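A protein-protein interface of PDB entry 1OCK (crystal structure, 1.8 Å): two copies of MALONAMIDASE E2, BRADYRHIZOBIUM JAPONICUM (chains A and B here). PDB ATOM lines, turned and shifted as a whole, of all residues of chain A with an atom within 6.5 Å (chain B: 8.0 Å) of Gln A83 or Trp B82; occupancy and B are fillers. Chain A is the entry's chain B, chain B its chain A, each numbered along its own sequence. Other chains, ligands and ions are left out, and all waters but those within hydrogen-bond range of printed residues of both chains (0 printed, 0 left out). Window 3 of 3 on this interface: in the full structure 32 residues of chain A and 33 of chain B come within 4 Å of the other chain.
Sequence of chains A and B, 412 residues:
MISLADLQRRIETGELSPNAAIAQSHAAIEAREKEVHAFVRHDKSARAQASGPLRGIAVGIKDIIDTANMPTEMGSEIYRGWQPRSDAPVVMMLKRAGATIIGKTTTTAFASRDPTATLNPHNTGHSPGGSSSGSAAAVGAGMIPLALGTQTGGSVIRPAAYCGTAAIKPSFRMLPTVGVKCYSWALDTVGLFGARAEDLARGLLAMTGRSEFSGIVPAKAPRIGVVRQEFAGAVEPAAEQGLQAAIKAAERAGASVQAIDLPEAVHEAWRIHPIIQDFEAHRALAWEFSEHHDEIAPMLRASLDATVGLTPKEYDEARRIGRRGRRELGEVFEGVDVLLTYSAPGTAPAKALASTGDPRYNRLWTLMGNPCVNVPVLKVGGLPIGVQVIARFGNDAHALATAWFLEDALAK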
ATOM      1  N   THR A  67      -8.539  -9.122  20.515  1.00  0.00           N
ATOM      2  CA  THR A  67      -9.503  -9.466  19.473  1.00  0.00           C
ATOM      3  C   THR A  67      -8.699  -9.317  18.187  1.00  0.00           C
ATOM      4  O   THR A  67      -7.835  -8.451  18.091  1.00  0.00           O
ATOM      5  CB  THR A  67     -10.760  -8.542  19.441  1.00  0.00           C
ATOM      6  OG1 THR A  67     -10.381  -7.172  19.615  1.00  0.00           O
ATOM      7  CG2 THR A  67     -11.745  -8.959  20.538  1.00  0.00           C
ATOM      8  N   ALA A  68      -8.962 -10.180  17.216  1.00  0.00           N
ATOM      9  CA  ALA A  68      -8.226 -10.153  15.955  1.00  0.00           C
ATOM     10  C   ALA A  68      -8.832  -9.221  14.911  1.00  0.00           C
ATOM     11  O   ALA A  68      -8.125  -8.730  14.033  1.00  0.00           O
ATOM     12  CB  ALA A  68      -8.139 -11.564  15.390  1.00  0.00           C
ATOM     13  N   ASN A  69     -10.137  -8.981  15.016  1.00  0.00           N
ATOM     14  CA  ASN A  69     -10.851  -8.136  14.063  1.00  0.00           C
ATOM     15  C   ASN A  69     -11.093  -6.702  14.529  1.00  0.00           C
ATOM     16  O   ASN A  69     -11.515  -5.859  13.739  1.00  0.00           O
ATOM     17  CB  ASN A  69     -12.187  -8.793  13.699  1.00  0.00           C
ATOM     18  CG  ASN A  69     -13.178  -8.780  14.847  1.00  0.00           C
ATOM     19  OD1 ASN A  69     -12.815  -8.994  16.007  1.00  0.00           O
ATOM     20  ND2 ASN A  69     -14.447  -8.538  14.527  1.00  0.00           N
ATOM     21  N   MET A  70     -10.841  -6.436  15.810  1.00  0.00           N
ATOM     22  CA  MET A  70     -11.014  -5.101  16.388  1.00  0.00           C
ATOM     23  C   MET A  70      -9.769  -4.757  17.202  1.00  0.00           C
ATOM     24  O   MET A  70      -9.117  -5.643  17.741  1.00  0.00           O
ATOM     25  CB  MET A  70     -12.224  -5.060  17.329  1.00  0.00           C
ATOM     26  CG  MET A  70     -13.578  -5.180  16.664  1.00  0.00           C
ATOM     27  SD  MET A  70     -14.888  -5.115  17.913  1.00  0.00           S
ATOM     28  CE  MET A  70     -15.051  -6.802  18.297  1.00  0.00           C
ATOM     29  N   PRO A  71      -9.433  -3.463  17.311  1.00  0.00           N
ATOM     30  CA  PRO A  71      -8.246  -3.096  18.085  1.00  0.00           C
ATOM     31  C   PRO A  71      -8.423  -3.407  19.572  1.00  0.00           C
ATOM     32  O   PRO A  71      -9.543  -3.579  20.055  1.00  0.00           O
ATOM     33  CB  PRO A  71      -8.115  -1.590  17.842  1.00  0.00           C
ATOM     34  CG  PRO A  71      -8.809  -1.376  16.518  1.00  0.00           C
ATOM     35  CD  PRO A  71     -10.002  -2.294  16.617  1.00  0.00           C
ATOM     36  N   THR A  72      -7.302  -3.486  20.280  1.00  0.00           N
ATOM     37  CA  THR A  72      -7.290  -3.733  21.722  1.00  0.00           C
ATOM     38  C   THR A  72      -6.319  -2.666  22.208  1.00  0.00           C
ATOM     39  O   THR A  72      -5.102  -2.849  22.164  1.00  0.00           O
ATOM     40  CB  THR A  72      -6.757  -5.134  22.042  1.00  0.00           C
ATOM     41  OG1 THR A  72      -7.529  -6.101  21.319  1.00  0.00           O
ATOM     42  CG2 THR A  72      -6.878  -5.425  23.538  1.00  0.00           C
ATOM     43  N   TYR A  79      -1.114   2.232  23.562  1.00  0.00           N
ATOM     44  CA  TYR A  79      -1.619   1.196  22.666  1.00  0.00           C
ATOM     45  C   TYR A  79      -2.695   1.683  21.704  1.00  0.00           C
ATOM     46  O   TYR A  79      -3.512   0.902  21.217  1.00  0.00           O
ATOM     47  CB  TYR A  79      -2.149   0.009  23.471  1.00  0.00           C
ATOM     48  CG  TYR A  79      -1.053  -0.817  24.083  1.00  0.00           C
ATOM     49  CD1 TYR A  79      -0.418  -0.411  25.261  1.00  0.00           C
ATOM     50  CD2 TYR A  79      -0.628  -2.001  23.476  1.00  0.00           C
ATOM     51  CE1 TYR A  79       0.614  -1.167  25.819  1.00  0.00           C
ATOM     52  CE2 TYR A  79       0.400  -2.759  24.026  1.00  0.00           C
ATOM     53  CZ  TYR A  79       1.015  -2.337  25.198  1.00  0.00           C
ATOM     54  OH  TYR A  79       2.028  -3.092  25.744  1.00  0.00           O
ATOM     55  N   GLY A  81      -4.483   2.353  18.537  1.00  0.00           N
ATOM     56  CA  GLY A  81      -4.355   1.704  17.243  1.00  0.00           C
ATOM     57  C   GLY A  81      -3.757   0.305  17.255  1.00  0.00           C
ATOM     58  O   GLY A  81      -3.549  -0.292  16.195  1.00  0.00           O
ATOM     59  N   TRP A  82      -3.477  -0.232  18.438  1.00  0.00           N
ATOM     60  CA  TRP A  82      -2.897  -1.566  18.526  1.00  0.00           C
ATOM     61  C   TRP A  82      -3.879  -2.643  18.093  1.00  0.00           C
ATOM     62  O   TRP A  82      -5.019  -2.687  18.565  1.00  0.00           O
ATOM     63  CB  TRP A  82      -2.420  -1.858  19.953  1.00  0.00           C
ATOM     64  CG  TRP A  82      -1.899  -3.251  20.110  1.00  0.00           C
ATOM     65  CD1 TRP A  82      -2.410  -4.235  20.908  1.00  0.00           C
ATOM     66  CD2 TRP A  82      -0.783  -3.830  19.424  1.00  0.00           C
ATOM     67  NE1 TRP A  82      -1.683  -5.392  20.761  1.00  0.00           N
ATOM     68  CE2 TRP A  82      -0.678  -5.173  19.857  1.00  0.00           C
ATOM     69  CE3 TRP A  82       0.137  -3.348  18.482  1.00  0.00           C
ATOM     70  CZ2 TRP A  82       0.313  -6.040  19.381  1.00  0.00           C
ATOM     71  CZ3 TRP A  82       1.124  -4.213  18.008  1.00  0.00           C
ATOM     72  CH2 TRP A  82       1.203  -5.543  18.459  1.00  0.00           C
ATOM     73  N   GLN A  83      -3.423  -3.516  17.197  1.00  0.00           N
ATOM     74  CA  GLN A  83      -4.249  -4.600  16.673  1.00  0.00           C
ATOM     75  C   GLN A  83      -3.623  -5.981  16.871  1.00  0.00           C
ATOM     76  O   GLN A  83      -2.704  -6.371  16.146  1.00  0.00           O
ATOM     77  CB  GLN A  83      -4.506  -4.376  15.176  1.00  0.00           C
ATOM     78  CG  GLN A  83      -5.425  -5.407  14.535  1.00  0.00           C
ATOM     79  CD  GLN A  83      -6.730  -5.570  15.293  1.00  0.00           C
ATOM     80  OE1 GLN A  83      -6.919  -6.540  16.033  1.00  0.00           O
ATOM     81  NE2 GLN A  83      -7.631  -4.615  15.124  1.00  0.00           N
ATOM     82  N   PRO A  84      -4.100  -6.733  17.874  1.00  0.00           N
ATOM     83  CA  PRO A  84      -3.558  -8.075  18.120  1.00  0.00           C
ATOM     84  C   PRO A  84      -3.791  -8.954  16.894  1.00  0.00           C
ATOM     85  O   PRO A  84      -4.731  -8.727  16.130  1.00  0.00           O
ATOM     86  CB  PRO A  84      -4.363  -8.562  19.325  1.00  0.00           C
ATOM     87  CG  PRO A  84      -4.673  -7.284  20.060  1.00  0.00           C
ATOM     88  CD  PRO A  84      -5.042  -6.338  18.937  1.00  0.00           C
ATOM     89  N   ARG A  85      -2.943  -9.960  16.720  1.00  0.00           N
ATOM     90  CA  ARG A  85      -3.059 -10.879  15.595  1.00  0.00           C
ATOM     91  C   ARG A  85      -4.170 -11.902  15.825  1.00  0.00           C
ATOM     92  O   ARG A  85      -4.907 -12.250  14.901  1.00  0.00           O
ATOM     93  CB  ARG A  85      -1.724 -11.602  15.382  1.00  0.00           C
ATOM     94  CG  ARG A  85      -1.733 -12.679  14.300  1.00  0.00           C
ATOM     95  CD  ARG A  85      -2.006 -12.108  12.915  1.00  0.00           C
ATOM     96  NE  ARG A  85      -1.715 -13.079  11.857  1.00  0.00           N
ATOM     97  CZ  ARG A  85      -2.554 -13.394  10.872  1.00  0.00           C
ATOM     98  NH1 ARG A  85      -3.749 -12.822  10.799  1.00  0.00           N
ATOM     99  NH2 ARG A  85      -2.191 -14.276   9.949  1.00  0.00           N
ATOM    100  N   SER A  86      -4.308 -12.366  17.063  1.00  0.00           N
ATOM    101  CA  SER A  86      -5.317 -13.373  17.370  1.00  0.00           C
ATOM    102  C   SER A  86      -6.352 -12.980  18.413  1.00  0.00           C
ATOM    103  O   SER A  86      -6.163 -12.035  19.181  1.00  0.00           O
ATOM    104  CB  SER A  86      -4.632 -14.653  17.849  1.00  0.00           C
ATOM    105  OG  SER A  86      -3.869 -14.405  19.018  1.00  0.00           O
ATOM    106  N   ARG B  41      16.523 -14.531  13.321  1.00  0.00           N
ATOM    107  CA  ARG B  41      17.046 -13.227  12.957  1.00  0.00           C
ATOM    108  C   ARG B  41      18.130 -12.798  13.931  1.00  0.00           C
ATOM    109  O   ARG B  41      17.958 -12.869  15.149  1.00  0.00           O
ATOM    110  CB  ARG B  41      15.923 -12.187  12.926  1.00  0.00           C
ATOM    111  CG  ARG B  41      15.219 -11.996  14.253  1.00  0.00           C
ATOM    112  CD  ARG B  41      13.979 -11.124  14.115  1.00  0.00           C
ATOM    113  NE  ARG B  41      13.012 -11.681  13.173  1.00  0.00           N
ATOM    114  CZ  ARG B  41      13.029 -11.467  11.860  1.00  0.00           C
ATOM    115  NH1 ARG B  41      13.968 -10.697  11.321  1.00  0.00           N
ATOM    116  NH2 ARG B  41      12.108 -12.021  11.085  1.00  0.00           N
ATOM    117  N   ASP B  63      11.891 -17.631  19.685  1.00  0.00           N
ATOM    118  CA  ASP B  63      10.915 -16.826  18.968  1.00  0.00           C
ATOM    119  C   ASP B  63       9.416 -16.971  19.213  1.00  0.00           C
ATOM    120  O   ASP B  63       8.624 -16.731  18.307  1.00  0.00           O
ATOM    121  CB  ASP B  63      11.199 -16.872  17.461  1.00  0.00           C
ATOM    122  CG  ASP B  63      10.804 -15.573  16.759  1.00  0.00           C
ATOM    123  OD1 ASP B  63      10.871 -14.503  17.401  1.00  0.00           O
ATOM    124  OD2 ASP B  63      10.446 -15.604  15.564  1.00  0.00           O
ATOM    125  N   ASP B  66       7.843 -12.489  23.038  1.00  0.00           N
ATOM    126  CA  ASP B  66       7.732 -11.131  22.505  1.00  0.00           C
ATOM    127  C   ASP B  66       8.926 -10.198  22.652  1.00  0.00           C
ATOM    128  O   ASP B  66       9.528 -10.090  23.724  1.00  0.00           O
ATOM    129  CB  ASP B  66       6.528 -10.403  23.121  1.00  0.00           C
ATOM    130  CG  ASP B  66       5.197 -10.938  22.637  1.00  0.00           C
ATOM    131  OD1 ASP B  66       5.174 -11.789  21.725  1.00  0.00           O
ATOM    132  OD2 ASP B  66       4.167 -10.487  23.179  1.00  0.00           O
ATOM    133  N   THR B  67       9.237  -9.518  21.552  1.00  0.00           N
ATOM    134  CA  THR B  67      10.288  -8.510  21.495  1.00  0.00           C
ATOM    135  C   THR B  67       9.651  -7.355  20.735  1.00  0.00           C
ATOM    136  O   THR B  67       8.903  -7.573  19.783  1.00  0.00           O
ATOM    137  CB  THR B  67      11.556  -8.989  20.745  1.00  0.00           C
ATOM    138  OG1 THR B  67      11.189  -9.658  19.533  1.00  0.00           O
ATOM    139  CG2 THR B  67      12.367  -9.915  21.627  1.00  0.00           C
ATOM    140  N   MET B  70      12.122  -6.512  17.377  1.00  0.00           N
ATOM    141  CA  MET B  70      12.323  -7.597  16.421  1.00  0.00           C
ATOM    142  C   MET B  70      11.043  -8.405  16.308  1.00  0.00           C
ATOM    143  O   MET B  70      10.299  -8.537  17.276  1.00  0.00           O
ATOM    144  CB  MET B  70      13.433  -8.546  16.881  1.00  0.00           C
ATOM    145  CG  MET B  70      14.842  -8.030  16.746  1.00  0.00           C
ATOM    146  SD  MET B  70      15.981  -9.291  17.356  1.00  0.00           S
ATOM    147  CE  MET B  70      15.984  -8.922  19.078  1.00  0.00           C
ATOM    148  N   PRO B  71      10.768  -8.957  15.120  1.00  0.00           N
ATOM    149  CA  PRO B  71       9.553  -9.754  14.944  1.00  0.00           C
ATOM    150  C   PRO B  71       9.549 -10.972  15.865  1.00  0.00           C
ATOM    151  O   PRO B  71      10.591 -11.413  16.340  1.00  0.00           O
ATOM    152  CB  PRO B  71       9.617 -10.153  13.472  1.00  0.00           C
ATOM    153  CG  PRO B  71      10.292  -8.963  12.842  1.00  0.00           C
ATOM    154  CD  PRO B  71      11.414  -8.693  13.821  1.00  0.00           C
ATOM    155  N   THR B  72       8.358 -11.491  16.129  1.00  0.00           N
ATOM    156  CA  THR B  72       8.183 -12.683  16.953  1.00  0.00           C
ATOM    157  C   THR B  72       7.257 -13.500  16.072  1.00  0.00           C
ATOM    158  O   THR B  72       6.043 -13.286  16.051  1.00  0.00           O
ATOM    159  CB  THR B  72       7.527 -12.328  18.289  1.00  0.00           C
ATOM    160  OG1 THR B  72       8.321 -11.324  18.936  1.00  0.00           O
ATOM    161  CG2 THR B  72       7.446 -13.550  19.188  1.00  0.00           C
ATOM    162  N   GLU B  73       7.848 -14.427  15.323  1.00  0.00           N
ATOM    163  CA  GLU B  73       7.093 -15.219  14.365  1.00  0.00           C
ATOM    164  C   GLU B  73       6.562 -16.582  14.791  1.00  0.00           C
ATOM    165  O   GLU B  73       5.956 -17.286  13.990  1.00  0.00           O
ATOM    166  CB  GLU B  73       7.921 -15.317  13.083  1.00  0.00           C
ATOM    167  CG  GLU B  73       8.361 -13.927  12.609  1.00  0.00           C
ATOM    168  CD  GLU B  73       9.178 -13.945  11.332  1.00  0.00           C
ATOM    169  OE1 GLU B  73      10.188 -14.676  11.282  1.00  0.00           O
ATOM    170  OE2 GLU B  73       8.812 -13.215  10.382  1.00  0.00           O
ATOM    171  N   MET B  74       6.781 -16.954  16.050  1.00  0.00           N
ATOM    172  CA  MET B  74       6.252 -18.217  16.569  1.00  0.00           C
ATOM    173  C   MET B  74       6.618 -19.469  15.769  1.00  0.00           C
ATOM    174  O   MET B  74       6.015 -20.523  15.970  1.00  0.00           O
ATOM    175  CB  MET B  74       4.722 -18.135  16.643  1.00  0.00           C
ATOM    176  CG  MET B  74       4.166 -16.778  17.054  1.00  0.00           C
ATOM    177  SD  MET B  74       4.677 -16.270  18.701  1.00  0.00           S
ATOM    178  CE  MET B  74       3.903 -14.642  18.802  1.00  0.00           C
ATOM    179  N   SER B  76       5.931 -20.028  12.863  1.00  0.00           N
ATOM    180  CA  SER B  76       4.781 -20.304  12.009  1.00  0.00           C
ATOM    181  C   SER B  76       4.573 -19.260  10.914  1.00  0.00           C
ATOM    182  O   SER B  76       4.788 -18.064  11.123  1.00  0.00           O
ATOM    183  CB  SER B  76       3.519 -20.383  12.875  1.00  0.00           C
ATOM    184  OG  SER B  76       2.347 -20.484  12.091  1.00  0.00           O
ATOM    185  N   GLU B  77       4.140 -19.721   9.746  1.00  0.00           N
ATOM    186  CA  GLU B  77       3.889 -18.819   8.627  1.00  0.00           C
ATOM    187  C   GLU B  77       2.724 -17.901   8.976  1.00  0.00           C
ATOM    188  O   GLU B  77       2.566 -16.836   8.394  1.00  0.00           O
ATOM    189  CB  GLU B  77       3.543 -19.615   7.371  1.00  0.00           C
ATOM    190  CG  GLU B  77       4.631 -20.566   6.908  1.00  0.00           C
ATOM    191  CD  GLU B  77       4.184 -21.414   5.731  1.00  0.00           C
ATOM    192  OE1 GLU B  77       3.208 -22.185   5.889  1.00  0.00           O
ATOM    193  OE2 GLU B  77       4.804 -21.310   4.648  1.00  0.00           O
ATOM    194  N   ILE B  78       1.904 -18.322   9.931  1.00  0.00           N
ATOM    195  CA  ILE B  78       0.758 -17.522  10.337  1.00  0.00           C
ATOM    196  C   ILE B  78       1.207 -16.198  10.949  1.00  0.00           C
ATOM    197  O   ILE B  78       0.521 -15.183  10.824  1.00  0.00           O
ATOM    198  CB  ILE B  78      -0.113 -18.294  11.354  1.00  0.00           C
ATOM    199  CG1 ILE B  78      -0.652 -19.573  10.701  1.00  0.00           C
ATOM    200  CG2 ILE B  78      -1.253 -17.404  11.850  1.00  0.00           C
ATOM    201  CD1 ILE B  78      -1.242 -20.575  11.682  1.00  0.00           C
ATOM    202  N   TYR B  79       2.370 -16.204  11.595  1.00  0.00           N
ATOM    203  CA  TYR B  79       2.888 -14.997  12.230  1.00  0.00           C
ATOM    204  C   TYR B  79       4.081 -14.365  11.526  1.00  0.00           C
ATOM    205  O   TYR B  79       4.848 -13.623  12.139  1.00  0.00           O
ATOM    206  CB  TYR B  79       3.252 -15.274  13.691  1.00  0.00           C
ATOM    207  CG  TYR B  79       2.049 -15.463  14.583  1.00  0.00           C
ATOM    208  CD1 TYR B  79       1.284 -16.629  14.525  1.00  0.00           C
ATOM    209  CD2 TYR B  79       1.664 -14.464  15.475  1.00  0.00           C
ATOM    210  CE1 TYR B  79       0.160 -16.793  15.337  1.00  0.00           C
ATOM    211  CE2 TYR B  79       0.547 -14.616  16.288  1.00  0.00           C
ATOM    212  CZ  TYR B  79      -0.200 -15.777  16.216  1.00  0.00           C
ATOM    213  OH  TYR B  79      -1.303 -15.914  17.024  1.00  0.00           O
ATOM    214  N   ARG B  80       4.231 -14.649  10.238  1.00  0.00           N
ATOM    215  CA  ARG B  80       5.330 -14.077   9.468  1.00  0.00           C
ATOM    216  C   ARG B  80       5.286 -12.555   9.573  1.00  0.00           C
ATOM    217  O   ARG B  80       4.256 -11.940   9.303  1.00  0.00           O
ATOM    218  CB  ARG B  80       5.202 -14.483   8.002  1.00  0.00           C
ATOM    219  CG  ARG B  80       6.266 -13.903   7.090  1.00  0.00           C
ATOM    220  CD  ARG B  80       5.932 -14.228   5.641  1.00  0.00           C
ATOM    221  NE  ARG B  80       7.057 -13.994   4.739  1.00  0.00           N
ATOM    222  CZ  ARG B  80       7.035 -14.259   3.436  1.00  0.00           C
ATOM    223  NH1 ARG B  80       5.941 -14.763   2.877  1.00  0.00           N
ATOM    224  NH2 ARG B  80       8.112 -14.033   2.694  1.00  0.00           N
ATOM    225  N   GLY B  81       6.404 -11.954   9.964  1.00  0.00           N
ATOM    226  CA  GLY B  81       6.463 -10.507  10.088  1.00  0.00           C
ATOM    227  C   GLY B  81       5.738  -9.909  11.286  1.00  0.00           C
ATOM    228  O   GLY B  81       5.735  -8.687  11.455  1.00  0.00           O
ATOM    229  N   TRP B  82       5.125 -10.749  12.118  1.00  0.00           N
ATOM    230  CA  TRP B  82       4.407 -10.259  13.297  1.00  0.00           C
ATOM    231  C   TRP B  82       5.334  -9.472  14.220  1.00  0.00           C
ATOM    232  O   TRP B  82       6.395  -9.963  14.627  1.00  0.00           O
ATOM    233  CB  TRP B  82       3.774 -11.425  14.074  1.00  0.00           C
ATOM    234  CG  TRP B  82       3.115 -11.010  15.373  1.00  0.00           C
ATOM    235  CD1 TRP B  82       3.451 -11.425  16.633  1.00  0.00           C
ATOM    236  CD2 TRP B  82       2.037 -10.075  15.534  1.00  0.00           C
ATOM    237  NE1 TRP B  82       2.654 -10.802  17.566  1.00  0.00           N
ATOM    238  CE2 TRP B  82       1.781  -9.966  16.921  1.00  0.00           C
ATOM    239  CE3 TRP B  82       1.267  -9.314  14.643  1.00  0.00           C
ATOM    240  CZ2 TRP B  82       0.784  -9.127  17.439  1.00  0.00           C
ATOM    241  CZ3 TRP B  82       0.273  -8.478  15.158  1.00  0.00           C
ATOM    242  CH2 TRP B  82       0.046  -8.391  16.545  1.00  0.00           C
ATOM    243  N   GLN B  83       4.918  -8.256  14.558  1.00  0.00           N
ATOM    244  CA  GLN B  83       5.709  -7.385  15.419  1.00  0.00           C
ATOM    245  C   GLN B  83       4.990  -6.972  16.698  1.00  0.00           C
ATOM    246  O   GLN B  83       4.142  -6.073  16.695  1.00  0.00           O
ATOM    247  CB  GLN B  83       6.122  -6.126  14.646  1.00  0.00           C
ATOM    248  CG  GLN B  83       7.051  -5.195  15.409  1.00  0.00           C
ATOM    249  CD  GLN B  83       8.234  -5.926  16.003  1.00  0.00           C
ATOM    250  OE1 GLN B  83       8.229  -6.291  17.182  1.00  0.00           O
ATOM    251  NE2 GLN B  83       9.253  -6.157  15.187  1.00  0.00           N
ATOM    252  N   PRO B  84       5.308  -7.635  17.815  1.00  0.00           N
ATOM    253  CA  PRO B  84       4.648  -7.263  19.070  1.00  0.00           C
ATOM    254  C   PRO B  84       4.956  -5.802  19.388  1.00  0.00           C
ATOM    255  O   PRO B  84       5.971  -5.254  18.936  1.00  0.00           O
ATOM    256  CB  PRO B  84       5.281  -8.213  20.079  1.00  0.00           C
ATOM    257  CG  PRO B  84       5.501  -9.447  19.264  1.00  0.00           C
ATOM    258  CD  PRO B  84       6.068  -8.888  17.971  1.00  0.00           C
ATOM    259  N   ARG B  85       4.080  -5.176  20.167  1.00  0.00           N
ATOM    260  CA  ARG B  85       4.260  -3.785  20.559  1.00  0.00           C
ATOM    261  C   ARG B  85       5.286  -3.697  21.687  1.00  0.00           C
ATOM    262  O   ARG B  85       6.109  -2.783  21.725  1.00  0.00           O
ATOM    263  CB  ARG B  85       2.923  -3.205  21.040  1.00  0.00           C
ATOM    264  CG  ARG B  85       2.988  -1.798  21.648  1.00  0.00           C
ATOM    265  CD  ARG B  85       3.071  -0.712  20.585  1.00  0.00           C
ATOM    266  NE  ARG B  85       2.933   0.632  21.147  1.00  0.00           N
ATOM    267  CZ  ARG B  85       3.901   1.545  21.161  1.00  0.00           C
ATOM    268  NH1 ARG B  85       5.089   1.263  20.644  1.00  0.00           N
ATOM    269  NH2 ARG B  85       3.681   2.743  21.687  1.00  0.00           N
ATOM    270  N   LYS B 104      16.625 -13.488  17.799  1.00  0.00           N
ATOM    271  CA  LYS B 104      15.563 -14.433  18.134  1.00  0.00           C
ATOM    272  C   LYS B 104      16.000 -15.809  17.646  1.00  0.00           C
ATOM    273  O   LYS B 104      16.316 -15.981  16.467  1.00  0.00           O
ATOM    274  CB  LYS B 104      14.247 -14.039  17.451  1.00  0.00           C
ATOM    275  CG  LYS B 104      13.793 -12.594  17.705  1.00  0.00           C
ATOM    276  CD  LYS B 104      13.658 -12.254  19.194  1.00  0.00           C
ATOM    277  CE  LYS B 104      12.529 -13.030  19.866  1.00  0.00           C
ATOM    278  NZ  LYS B 104      11.188 -12.650  19.341  1.00  0.00           N
ATOM    279  N   LYS B 181       4.048 -16.949  23.877  1.00  0.00           N
ATOM    280  CA  LYS B 181       2.990 -17.708  23.212  1.00  0.00           C
ATOM    281  C   LYS B 181       2.644 -18.955  24.017  1.00  0.00           C
ATOM    282  O   LYS B 181       3.510 -19.782  24.311  1.00  0.00           O
ATOM    283  CB  LYS B 181       3.420 -18.092  21.791  1.00  0.00           C
ATOM    284  CG  LYS B 181       2.306 -18.701  20.943  1.00  0.00           C
ATOM    285  CD  LYS B 181       1.162 -17.718  20.718  1.00  0.00           C
ATOM    286  CE  LYS B 181       0.097 -18.334  19.819  1.00  0.00           C
ATOM    287  NZ  LYS B 181      -1.156 -17.546  19.800  1.00  0.00           N
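O of Ile B78 sits at hydrogen-bond distance from NH2 of Arg A85 (3.0 Å).
O of Thr A67 lies close to OE1 of Gln A83 (3.0 Å).
N of Ile B78 lies close to OG of Ser B76, 3.1 Å away.
OE1 of Gln B83 lies close to O of Thr B67 (3.0 Å).
The backbone carbonyl oxygen of Met B70 sits close to the side-chain amide oxygen of Gln B83.
O of Ala A68 sits close to OE1 of Gln A83 (3.2 Å).
The backbone carbonyl oxygen of Trp B82 lies within hydrogen-bond range of the backbone NH of Thr B72 (2.9 Å).
Tyr A79 touches Arg B85.
Trp A82 touches Trp B82 (CH2 to CH2, 3.6 Å).
CH2 of Trp A82 touches O of Gln B83, at 3.5 Å.
Pro B84 touches Trp A82.
Trp A82 touches Arg B85.
O of Gln A83 touches CH2 of Trp B82, 3.4 Å away.
Pro A84 touches Trp B82.
Tyr B79 touches Arg A85 (CE2 to CG, 3.6 Å).
Trp B82 touches Arg A85 (CH2 to N, 3.4 Å).
OG of Ser A86 touches OH of Tyr B79, at 3.6 Å.
Of the printed residues of chain B, Tyr A79 touches Arg B85.
Gln A83 touches just one residue of chain B: Trp B82 (3.4 Å).
Pro A84 touches just one residue of chain B: Trp B82 (3.9 Å).
Of the printed residues of chain B, Ser A86 touches Tyr B79.
Thr B67 touches none of the printed residues of chain A.
Met B74 touches none of the printed residues of chain A.
Of the printed residues of chain A, Tyr B79 touches Arg A85 (3.6 Å) and Ser A86 (3.6 Å).
Printed residues of chain A within 4 Å of Gln B83: Trp A82.
Of the printed residues of chain A, Arg B85 touches Tyr A79 (3.6 Å) and Trp A82 (3.4 Å).
Of the 21 printed residues of chain B, 6 touch a printed residue of chain A.
Along chain B the printed residues that touch a printed residue of chain A span positions 78 to 85.
Hydrophobic or aromatic side chains of chain A that line the printed part of chain B: Tyr A79 and Trp A82.
Among the printed residues, 11 pairs touch across the chains.
Among the printed residues, no Asp or Glu carboxylate lies within 4 Å of a Lys or Arg side-chain nitrogen of the other chain.
Trp B82 touches its own counterpart, Trp A82.
Trp A82 touches Gln B83, and with the chains exchanged Gln A83 touches Trp B82.
Trp A82 touches Pro B84, and with the chains exchanged Pro A84 touches Trp B82.
Trp A82 touches Arg B85, and with the chains exchanged Arg A85 touches Trp B82.
Positions printed for both chains: 67, 70, 71, 72, 79, 81, 82, 83, 84 and 85.
Of the 11 pairs that touch across the chains among the printed residues, 9 have their exchanged pair printed and touching as well.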
